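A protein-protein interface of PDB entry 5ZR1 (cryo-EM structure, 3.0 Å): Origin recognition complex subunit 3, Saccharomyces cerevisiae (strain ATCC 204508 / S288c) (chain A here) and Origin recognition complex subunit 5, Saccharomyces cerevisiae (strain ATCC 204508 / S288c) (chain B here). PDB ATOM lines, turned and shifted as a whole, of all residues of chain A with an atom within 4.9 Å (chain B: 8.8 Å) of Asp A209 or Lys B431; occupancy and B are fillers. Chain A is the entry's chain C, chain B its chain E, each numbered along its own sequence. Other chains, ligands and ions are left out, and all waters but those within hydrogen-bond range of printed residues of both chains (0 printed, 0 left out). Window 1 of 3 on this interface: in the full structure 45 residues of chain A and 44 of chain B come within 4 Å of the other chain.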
ATOM      1  N   ASP A 207      23.947  26.167 -16.151  1.00  0.00           N
ATOM      2  CA  ASP A 207      22.867  26.176 -17.129  1.00  0.00           C
ATOM      3  C   ASP A 207      22.286  24.770 -17.140  1.00  0.00           C
ATOM      4  O   ASP A 207      22.599  23.943 -17.994  1.00  0.00           O
ATOM      5  CB  ASP A 207      23.351  26.614 -18.498  1.00  0.00           C
ATOM      6  CG  ASP A 207      23.791  28.065 -18.520  1.00  0.00           C
ATOM      7  OD1 ASP A 207      23.246  28.864 -17.732  1.00  0.00           O
ATOM      8  OD2 ASP A 207      24.689  28.404 -19.319  1.00  0.00           O
ATOM      9  N   VAL A 208      21.407  24.514 -16.173  1.00  0.00           N
ATOM     10  CA  VAL A 208      20.837  23.185 -15.991  1.00  0.00           C
ATOM     11  C   VAL A 208      19.734  22.909 -17.002  1.00  0.00           C
ATOM     12  O   VAL A 208      19.380  21.748 -17.230  1.00  0.00           O
ATOM     13  CB  VAL A 208      20.435  23.110 -14.505  1.00  0.00           C
ATOM     14  CG1 VAL A 208      19.400  24.122 -14.224  1.00  0.00           C
ATOM     15  CG2 VAL A 208      19.960  21.734 -14.087  1.00  0.00           C
ATOM     16  N   ASP A 209      19.219  23.938 -17.667  1.00  0.00           N
ATOM     17  CA  ASP A 209      18.343  23.713 -18.806  1.00  0.00           C
ATOM     18  C   ASP A 209      19.108  23.359 -20.071  1.00  0.00           C
ATOM     19  O   ASP A 209      18.489  22.930 -21.050  1.00  0.00           O
ATOM     20  CB  ASP A 209      17.480  24.949 -19.049  1.00  0.00           C
ATOM     21  CG  ASP A 209      16.457  25.157 -17.959  1.00  0.00           C
ATOM     22  OD1 ASP A 209      15.961  24.153 -17.410  1.00  0.00           O
ATOM     23  OD2 ASP A 209      16.168  26.323 -17.629  1.00  0.00           O
ATOM     24  N   SER A 210      20.429  23.524 -20.071  1.00  0.00           N
ATOM     25  CA  SER A 210      21.267  23.167 -21.206  1.00  0.00           C
ATOM     26  C   SER A 210      22.016  21.858 -21.004  1.00  0.00           C
ATOM     27  O   SER A 210      22.468  21.266 -21.987  1.00  0.00           O
ATOM     28  CB  SER A 210      22.276  24.285 -21.487  1.00  0.00           C
ATOM     29  OG  SER A 210      21.617  25.490 -21.829  1.00  0.00           O
ATOM     30  N   ILE A 211      22.161  21.403 -19.758  1.00  0.00           N
ATOM     31  CA  ILE A 211      22.746  20.096 -19.496  1.00  0.00           C
ATOM     32  C   ILE A 211      21.731  19.024 -19.881  1.00  0.00           C
ATOM     33  O   ILE A 211      20.519  19.279 -19.944  1.00  0.00           O
ATOM     34  CB  ILE A 211      23.167  19.994 -18.015  1.00  0.00           C
ATOM     35  CG1 ILE A 211      24.182  18.876 -17.781  1.00  0.00           C
ATOM     36  CG2 ILE A 211      21.978  19.759 -17.106  1.00  0.00           C
ATOM     37  CD1 ILE A 211      24.763  18.890 -16.390  1.00  0.00           C
ATOM     38  N   PHE A 213      19.826  15.588 -18.842  1.00  0.00           N
ATOM     39  CA  PHE A 213      19.364  15.151 -17.540  1.00  0.00           C
ATOM     40  C   PHE A 213      19.630  13.682 -17.278  1.00  0.00           C
ATOM     41  O   PHE A 213      19.307  13.202 -16.196  1.00  0.00           O
ATOM     42  CB  PHE A 213      17.876  15.453 -17.396  1.00  0.00           C
ATOM     43  CG  PHE A 213      17.568  16.914 -17.362  1.00  0.00           C
ATOM     44  CD1 PHE A 213      17.635  17.621 -16.177  1.00  0.00           C
ATOM     45  CD2 PHE A 213      17.241  17.590 -18.525  1.00  0.00           C
ATOM     46  CE1 PHE A 213      17.357  18.965 -16.149  1.00  0.00           C
ATOM     47  CE2 PHE A 213      16.966  18.934 -18.501  1.00  0.00           C
ATOM     48  CZ  PHE A 213      17.025  19.618 -17.316  1.00  0.00           C
ATOM     49  N   ASN A 239      20.271  26.359 -11.064  1.00  0.00           N
ATOM     50  CA  ASN A 239      19.902  27.619 -11.708  1.00  0.00           C
ATOM     51  C   ASN A 239      18.931  27.342 -12.855  1.00  0.00           C
ATOM     52  O   ASN A 239      19.262  27.454 -14.036  1.00  0.00           O
ATOM     53  CB  ASN A 239      21.143  28.337 -12.210  1.00  0.00           C
ATOM     54  CG  ASN A 239      22.034  28.814 -11.103  1.00  0.00           C
ATOM     55  OD1 ASN A 239      23.086  28.244 -10.849  1.00  0.00           O
ATOM     56  ND2 ASN A 239      21.655  29.915 -10.483  1.00  0.00           N
ATOM     57  N   ILE A 240      17.710  26.967 -12.489  1.00  0.00           N
ATOM     58  CA  ILE A 240      16.698  26.625 -13.484  1.00  0.00           C
ATOM     59  C   ILE A 240      16.155  27.911 -14.107  1.00  0.00           C
ATOM     60  O   ILE A 240      15.475  28.708 -13.460  1.00  0.00           O
ATOM     61  CB  ILE A 240      15.595  25.734 -12.892  1.00  0.00           C
ATOM     62  CG1 ILE A 240      15.109  26.219 -11.529  1.00  0.00           C
ATOM     63  CG2 ILE A 240      16.086  24.319 -12.719  1.00  0.00           C
ATOM     64  CD1 ILE A 240      13.985  25.382 -10.984  1.00  0.00           C
ATOM     65  N   ASN A 241      16.505  28.129 -15.376  1.00  0.00           N
ATOM     66  CA  ASN A 241      16.193  29.383 -16.053  1.00  0.00           C
ATOM     67  C   ASN A 241      14.715  29.481 -16.397  1.00  0.00           C
ATOM     68  O   ASN A 241      14.170  30.583 -16.500  1.00  0.00           O
ATOM     69  CB  ASN A 241      17.037  29.496 -17.327  1.00  0.00           C
ATOM     70  CG  ASN A 241      17.069  30.901 -17.902  1.00  0.00           C
ATOM     71  OD1 ASN A 241      16.562  31.850 -17.310  1.00  0.00           O
ATOM     72  ND2 ASN A 241      17.659  31.033 -19.085  1.00  0.00           N
ATOM     73  N   THR A 242      14.046  28.348 -16.575  1.00  0.00           N
ATOM     74  CA  THR A 242      12.689  28.347 -17.102  1.00  0.00           C
ATOM     75  C   THR A 242      11.644  28.026 -16.044  1.00  0.00           C
ATOM     76  O   THR A 242      10.726  28.815 -15.805  1.00  0.00           O
ATOM     77  CB  THR A 242      12.578  27.324 -18.231  1.00  0.00           C
ATOM     78  OG1 THR A 242      12.781  26.007 -17.703  1.00  0.00           O
ATOM     79  CG2 THR A 242      13.611  27.588 -19.267  1.00  0.00           C
ATOM     80  N   ILE A 247      11.711  20.301 -15.200  1.00  0.00           N
ATOM     81  CA  ILE A 247      12.838  19.545 -14.669  1.00  0.00           C
ATOM     82  C   ILE A 247      12.373  18.218 -14.091  1.00  0.00           C
ATOM     83  O   ILE A 247      13.031  17.187 -14.263  1.00  0.00           O
ATOM     84  CB  ILE A 247      13.586  20.391 -13.626  1.00  0.00           C
ATOM     85  CG1 ILE A 247      13.942  21.747 -14.222  1.00  0.00           C
ATOM     86  CG2 ILE A 247      14.849  19.698 -13.161  1.00  0.00           C
ATOM     87  CD1 ILE A 247      14.816  21.691 -15.439  1.00  0.00           C
ATOM     88  N   TYR B 322       5.815  28.352 -17.719  1.00  0.00           N
ATOM     89  CA  TYR B 322       7.003  29.100 -18.100  1.00  0.00           C
ATOM     90  C   TYR B 322       6.770  30.596 -17.931  1.00  0.00           C
ATOM     91  O   TYR B 322       5.635  31.078 -17.984  1.00  0.00           O
ATOM     92  CB  TYR B 322       7.418  28.822 -19.548  1.00  0.00           C
ATOM     93  CG  TYR B 322       7.940  27.433 -19.821  1.00  0.00           C
ATOM     94  CD1 TYR B 322       9.198  27.048 -19.392  1.00  0.00           C
ATOM     95  CD2 TYR B 322       7.208  26.534 -20.572  1.00  0.00           C
ATOM     96  CE1 TYR B 322       9.684  25.780 -19.654  1.00  0.00           C
ATOM     97  CE2 TYR B 322       7.682  25.269 -20.829  1.00  0.00           C
ATOM     98  CZ  TYR B 322       8.919  24.897 -20.370  1.00  0.00           C
ATOM     99  OH  TYR B 322       9.396  23.638 -20.637  1.00  0.00           O
ATOM    100  N   LEU B 332       6.229  28.620 -29.509  1.00  0.00           N
ATOM    101  CA  LEU B 332       6.137  27.195 -29.222  1.00  0.00           C
ATOM    102  C   LEU B 332       4.811  26.608 -29.672  1.00  0.00           C
ATOM    103  O   LEU B 332       4.753  25.421 -30.007  1.00  0.00           O
ATOM    104  CB  LEU B 332       6.306  26.917 -27.731  1.00  0.00           C
ATOM    105  CG  LEU B 332       7.682  26.936 -27.092  1.00  0.00           C
ATOM    106  CD1 LEU B 332       7.544  26.790 -25.606  1.00  0.00           C
ATOM    107  CD2 LEU B 332       8.477  25.787 -27.634  1.00  0.00           C
ATOM    108  N   LEU B 424      13.252  33.099 -30.982  1.00  0.00           N
ATOM    109  CA  LEU B 424      13.310  31.751 -31.528  1.00  0.00           C
ATOM    110  C   LEU B 424      14.657  31.116 -31.231  1.00  0.00           C
ATOM    111  O   LEU B 424      14.740  29.901 -31.038  1.00  0.00           O
ATOM    112  CB  LEU B 424      13.063  31.790 -33.034  1.00  0.00           C
ATOM    113  CG  LEU B 424      12.517  30.589 -33.809  1.00  0.00           C
ATOM    114  CD1 LEU B 424      11.929  31.127 -35.091  1.00  0.00           C
ATOM    115  CD2 LEU B 424      13.510  29.478 -34.104  1.00  0.00           C
ATOM    116  N   SER B 425      15.713  31.924 -31.194  1.00  0.00           N
ATOM    117  CA  SER B 425      17.035  31.432 -30.844  1.00  0.00           C
ATOM    118  C   SER B 425      17.171  31.186 -29.351  1.00  0.00           C
ATOM    119  O   SER B 425      17.886  30.268 -28.946  1.00  0.00           O
ATOM    120  CB  SER B 425      18.094  32.425 -31.306  1.00  0.00           C
ATOM    121  OG  SER B 425      19.385  31.984 -30.943  1.00  0.00           O
ATOM    122  N   GLU B 426      16.511  31.998 -28.525  1.00  0.00           N
ATOM    123  CA  GLU B 426      16.475  31.752 -27.087  1.00  0.00           C
ATOM    124  C   GLU B 426      15.664  30.511 -26.764  1.00  0.00           C
ATOM    125  O   GLU B 426      15.969  29.798 -25.805  1.00  0.00           O
ATOM    126  CB  GLU B 426      15.889  32.970 -26.372  1.00  0.00           C
ATOM    127  CG  GLU B 426      15.799  32.896 -24.852  1.00  0.00           C
ATOM    128  CD  GLU B 426      17.153  32.942 -24.158  1.00  0.00           C
ATOM    129  OE1 GLU B 426      18.139  33.385 -24.781  1.00  0.00           O
ATOM    130  OE2 GLU B 426      17.221  32.590 -22.964  1.00  0.00           O
ATOM    131  N   LEU B 427      14.651  30.224 -27.576  1.00  0.00           N
ATOM    132  CA  LEU B 427      13.822  29.049 -27.379  1.00  0.00           C
ATOM    133  C   LEU B 427      14.568  27.777 -27.757  1.00  0.00           C
ATOM    134  O   LEU B 427      14.201  26.693 -27.303  1.00  0.00           O
ATOM    135  CB  LEU B 427      12.558  29.211 -28.214  1.00  0.00           C
ATOM    136  CG  LEU B 427      11.247  28.508 -27.938  1.00  0.00           C
ATOM    137  CD1 LEU B 427      10.725  29.030 -26.627  1.00  0.00           C
ATOM    138  CD2 LEU B 427      10.294  28.854 -29.049  1.00  0.00           C
ATOM    139  N   HIS B 428      15.618  27.904 -28.568  1.00  0.00           N
ATOM    140  CA  HIS B 428      16.472  26.789 -28.944  1.00  0.00           C
ATOM    141  C   HIS B 428      17.563  26.518 -27.921  1.00  0.00           C
ATOM    142  O   HIS B 428      17.933  25.357 -27.713  1.00  0.00           O
ATOM    143  CB  HIS B 428      17.087  27.059 -30.315  1.00  0.00           C
ATOM    144  CG  HIS B 428      18.090  26.038 -30.743  1.00  0.00           C
ATOM    145  ND1 HIS B 428      19.444  26.218 -30.574  1.00  0.00           N
ATOM    146  CD2 HIS B 428      17.939  24.809 -31.287  1.00  0.00           C
ATOM    147  CE1 HIS B 428      20.086  25.157 -31.028  1.00  0.00           C
ATOM    148  NE2 HIS B 428      19.195  24.285 -31.463  1.00  0.00           N
ATOM    149  N   THR B 429      18.090  27.556 -27.270  1.00  0.00           N
ATOM    150  CA  THR B 429      19.106  27.347 -26.247  1.00  0.00           C
ATOM    151  C   THR B 429      18.516  26.784 -24.968  1.00  0.00           C
ATOM    152  O   THR B 429      19.247  26.198 -24.165  1.00  0.00           O
ATOM    153  CB  THR B 429      19.832  28.653 -25.938  1.00  0.00           C
ATOM    154  OG1 THR B 429      18.897  29.612 -25.435  1.00  0.00           O
ATOM    155  CG2 THR B 429      20.492  29.196 -27.190  1.00  0.00           C
ATOM    156  N   LEU B 430      17.215  26.947 -24.771  1.00  0.00           N
ATOM    157  CA  LEU B 430      16.484  26.427 -23.627  1.00  0.00           C
ATOM    158  C   LEU B 430      15.991  25.011 -23.856  1.00  0.00           C
ATOM    159  O   LEU B 430      15.262  24.483 -23.008  1.00  0.00           O
ATOM    160  CB  LEU B 430      15.310  27.357 -23.315  1.00  0.00           C
ATOM    161  CG  LEU B 430      15.477  28.510 -22.327  1.00  0.00           C
ATOM    162  CD1 LEU B 430      16.653  29.396 -22.621  1.00  0.00           C
ATOM    163  CD2 LEU B 430      14.216  29.351 -22.415  1.00  0.00           C
ATOM    164  N   LYS B 431      16.372  24.409 -24.991  1.00  0.00           N
ATOM    165  CA  LYS B 431      16.018  23.043 -25.391  1.00  0.00           C
ATOM    166  C   LYS B 431      14.506  22.856 -25.482  1.00  0.00           C
ATOM    167  O   LYS B 431      13.969  21.806 -25.131  1.00  0.00           O
ATOM    168  CB  LYS B 431      16.652  22.005 -24.462  1.00  0.00           C
ATOM    169  CG  LYS B 431      18.161  22.131 -24.356  1.00  0.00           C
ATOM    170  CD  LYS B 431      18.841  21.823 -25.674  1.00  0.00           C
ATOM    171  CE  LYS B 431      20.353  21.855 -25.529  1.00  0.00           C
ATOM    172  NZ  LYS B 431      20.858  23.241 -25.325  1.00  0.00           N
ATOM    173  N   LEU B 432      13.812  23.892 -25.957  1.00  0.00           N
ATOM    174  CA  LEU B 432      12.389  23.799 -26.243  1.00  0.00           C
ATOM    175  C   LEU B 432      12.107  23.628 -27.727  1.00  0.00           C
ATOM    176  O   LEU B 432      11.028  23.151 -28.084  1.00  0.00           O
ATOM    177  CB  LEU B 432      11.653  25.038 -25.722  1.00  0.00           C
ATOM    178  CG  LEU B 432      11.764  25.309 -24.217  1.00  0.00           C
ATOM    179  CD1 LEU B 432      10.972  26.540 -23.828  1.00  0.00           C
ATOM    180  CD2 LEU B 432      11.354  24.118 -23.383  1.00  0.00           C
ATOM    181  N   ILE B 433      13.048  24.008 -28.587  1.00  0.00           N
ATOM    182  CA  ILE B 433      13.049  23.660 -30.003  1.00  0.00           C
ATOM    183  C   ILE B 433      14.296  22.828 -30.256  1.00  0.00           C
ATOM    184  O   ILE B 433      15.382  23.171 -29.781  1.00  0.00           O
ATOM    185  CB  ILE B 433      13.044  24.910 -30.906  1.00  0.00           C
ATOM    186  CG1 ILE B 433      11.927  25.859 -30.510  1.00  0.00           C
ATOM    187  CG2 ILE B 433      12.816  24.528 -32.339  1.00  0.00           C
ATOM    188  CD1 ILE B 433      10.573  25.269 -30.630  1.00  0.00           C
ATOM    189  N   ALA B 434      14.148  21.731 -30.984  1.00  0.00           N
ATOM    190  CA  ALA B 434      15.280  20.871 -31.290  1.00  0.00           C
ATOM    191  C   ALA B 434      15.611  20.944 -32.773  1.00  0.00           C
ATOM    192  O   ALA B 434      14.837  21.449 -33.585  1.00  0.00           O
ATOM    193  CB  ALA B 434      14.992  19.425 -30.881  1.00  0.00           C
ATOM    194  N   THR B 435      16.793  20.437 -33.115  1.00  0.00           N
ATOM    195  CA  THR B 435      17.240  20.287 -34.493  1.00  0.00           C
ATOM    196  C   THR B 435      17.701  18.854 -34.710  1.00  0.00           C
ATOM    197  O   THR B 435      17.650  18.014 -33.808  1.00  0.00           O
ATOM    198  CB  THR B 435      18.394  21.239 -34.842  1.00  0.00           C
ATOM    199  OG1 THR B 435      19.506  20.981 -33.977  1.00  0.00           O
ATOM    200  CG2 THR B 435      17.988  22.681 -34.717  1.00  0.00           C
ATOM    201  N   TYR B 443      22.607  27.399 -37.920  1.00  0.00           N
ATOM    202  CA  TYR B 443      21.249  27.917 -38.036  1.00  0.00           C
ATOM    203  C   TYR B 443      20.961  28.398 -39.448  1.00  0.00           C
ATOM    204  O   TYR B 443      19.831  28.288 -39.934  1.00  0.00           O
ATOM    205  CB  TYR B 443      21.069  29.097 -37.084  1.00  0.00           C
ATOM    206  CG  TYR B 443      21.289  28.827 -35.618  1.00  0.00           C
ATOM    207  CD1 TYR B 443      20.250  28.407 -34.803  1.00  0.00           C
ATOM    208  CD2 TYR B 443      22.538  29.008 -35.046  1.00  0.00           C
ATOM    209  CE1 TYR B 443      20.449  28.173 -33.453  1.00  0.00           C
ATOM    210  CE2 TYR B 443      22.750  28.774 -33.702  1.00  0.00           C
ATOM    211  CZ  TYR B 443      21.704  28.358 -32.911  1.00  0.00           C
ATOM    212  OH  TYR B 443      21.920  28.127 -31.575  1.00  0.00           O
ATOM    213  N   LYS B 451      12.326  21.056 -34.860  1.00  0.00           N
ATOM    214  CA  LYS B 451      11.201  20.359 -34.261  1.00  0.00           C
ATOM    215  C   LYS B 451      11.064  20.818 -32.824  1.00  0.00           C
ATOM    216  O   LYS B 451      12.012  21.317 -32.218  1.00  0.00           O
ATOM    217  CB  LYS B 451      11.369  18.840 -34.331  1.00  0.00           C
ATOM    218  CG  LYS B 451      12.578  18.342 -33.588  1.00  0.00           C
ATOM    219  CD  LYS B 451      12.789  16.865 -33.786  1.00  0.00           C
ATOM    220  CE  LYS B 451      14.075  16.432 -33.125  1.00  0.00           C
ATOM    221  NZ  LYS B 451      14.367  15.004 -33.381  1.00  0.00           N
ATOM    222  N   VAL B 452       9.896  20.650 -32.296  1.00  0.00           N
ATOM    223  CA  VAL B 452       9.635  21.032 -30.918  1.00  0.00           C
ATOM    224  C   VAL B 452       9.929  19.830 -30.034  1.00  0.00           C
ATOM    225  O   VAL B 452       9.802  18.679 -30.461  1.00  0.00           O
ATOM    226  CB  VAL B 452       8.184  21.550 -30.771  1.00  0.00           C
ATOM    227  CG1 VAL B 452       7.162  20.439 -30.958  1.00  0.00           C
ATOM    228  CG2 VAL B 452       7.984  22.272 -29.461  1.00  0.00           C
ATOM    229  N   ASN B 453      10.425  20.071 -28.824  1.00  0.00           N
ATOM    230  CA  ASN B 453      10.386  19.041 -27.790  1.00  0.00           C
ATOM    231  C   ASN B 453       9.849  19.657 -26.498  1.00  0.00           C
ATOM    232  O   ASN B 453      10.583  19.977 -25.562  1.00  0.00           O
ATOM    233  CB  ASN B 453      11.761  18.347 -27.615  1.00  0.00           C
ATOM    234  CG  ASN B 453      12.900  19.313 -27.420  1.00  0.00           C
ATOM    235  OD1 ASN B 453      12.712  20.523 -27.424  1.00  0.00           O
ATOM    236  ND2 ASN B 453      14.091  18.776 -27.207  1.00  0.00           N
ATOM    237  N   VAL B 454       8.529  19.780 -26.446  1.00  0.00           N
ATOM    238  CA  VAL B 454       7.774  19.902 -25.206  1.00  0.00           C
ATOM    239  C   VAL B 454       6.643  18.892 -25.336  1.00  0.00           C
ATOM    240  O   VAL B 454       6.212  18.589 -26.457  1.00  0.00           O
ATOM    241  CB  VAL B 454       7.248  21.329 -24.953  1.00  0.00           C
ATOM    242  CG1 VAL B 454       8.380  22.287 -24.681  1.00  0.00           C
ATOM    243  CG2 VAL B 454       6.414  21.825 -26.116  1.00  0.00           C
ATOM    244  N   PRO B 455       6.172  18.304 -24.244  1.00  0.00           N
ATOM    245  CA  PRO B 455       5.015  17.411 -24.332  1.00  0.00           C
ATOM    246  C   PRO B 455       3.730  18.183 -24.600  1.00  0.00           C
ATOM    247  O   PRO B 455       3.692  19.414 -24.615  1.00  0.00           O
ATOM    248  CB  PRO B 455       4.991  16.736 -22.960  1.00  0.00           C
ATOM    249  CG  PRO B 455       6.390  16.832 -22.474  1.00  0.00           C
ATOM    250  CD  PRO B 455       6.896  18.139 -22.975  1.00  0.00           C
ATOM    251  N   ILE B 458       2.516  20.421 -21.627  1.00  0.00           N
ATOM    252  CA  ILE B 458       3.096  21.749 -21.473  1.00  0.00           C
ATOM    253  C   ILE B 458       2.471  22.738 -22.449  1.00  0.00           C
ATOM    254  O   ILE B 458       2.119  23.861 -22.070  1.00  0.00           O
ATOM    255  CB  ILE B 458       4.626  21.660 -21.614  1.00  0.00           C
ATOM    256  CG1 ILE B 458       5.226  21.073 -20.334  1.00  0.00           C
ATOM    257  CG2 ILE B 458       5.234  22.988 -21.981  1.00  0.00           C
ATOM    258  CD1 ILE B 458       6.702  20.812 -20.402  1.00  0.00           C
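The side-chain hydroxyl (OG) of Ser A210 lies within hydrogen-bond range of the backbone carbonyl oxygen (O) of Thr B429 (3.4 Å).
The side-chain carboxylate (OD2) of Asp A209 is in hydrogen-bond range of the backbone NH (N) of Asn A241, at 2.9 Å.
O of Lys B431 sits close to OD1 of Asn B453, at 2.9 Å.
The backbone NH (N) of Thr A242 sits at hydrogen-bond distance from the side-chain carboxylate (OD2) of Asp A209 (3.1 Å).
The side-chain hydroxyl of Thr B429 is in hydrogen-bond range of the backbone carbonyl oxygen of Glu B426.
Among the printed residues, merely in contact across the chains: Asp A209 with Lys B431 (3.4 Å), Thr A242 with Tyr B322 (3.6 Å) and Thr A242 with Leu B430 (3.7 Å).
No residue of chain B comes within 4 Å of Val A208.
Asp A209 touches just one residue of chain B: Lys B431.
Of chain B, only Thr B429 (3.4 Å) comes within 4 Å of Ser A210.
Printed residues of chain B within 4 Å of Thr A242: Tyr B322 (3.6 Å) and Leu B430 (3.7 Å).
Of the printed residues of chain A, Leu B430 touches Thr A242 (3.7 Å).
Of the printed residues of chain A, Lys B431 touches Asp A209.
The nearest printed residue of chain B that does not touch Thr A242 is Leu B432 (5.4 Å).
Printed residues of chain A that touch a printed residue of chain B: Asp A209, Ser A210 and Thr A242.
Of the 21 printed residues of chain B, 4 touch a printed residue of chain A.
Printed residues of chain B that touch a printed residue of chain A: Tyr B322, Thr B429, Leu B430 and Lys B431.
Hydrophobic or aromatic side chains of chain B within 4 Å of the printed part of chain A: Tyr B322 and Leu B430.
Among the printed residues, no Asp or Glu carboxylate lies within 4 Å of a Lys or Arg side-chain nitrogen of the other chain.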
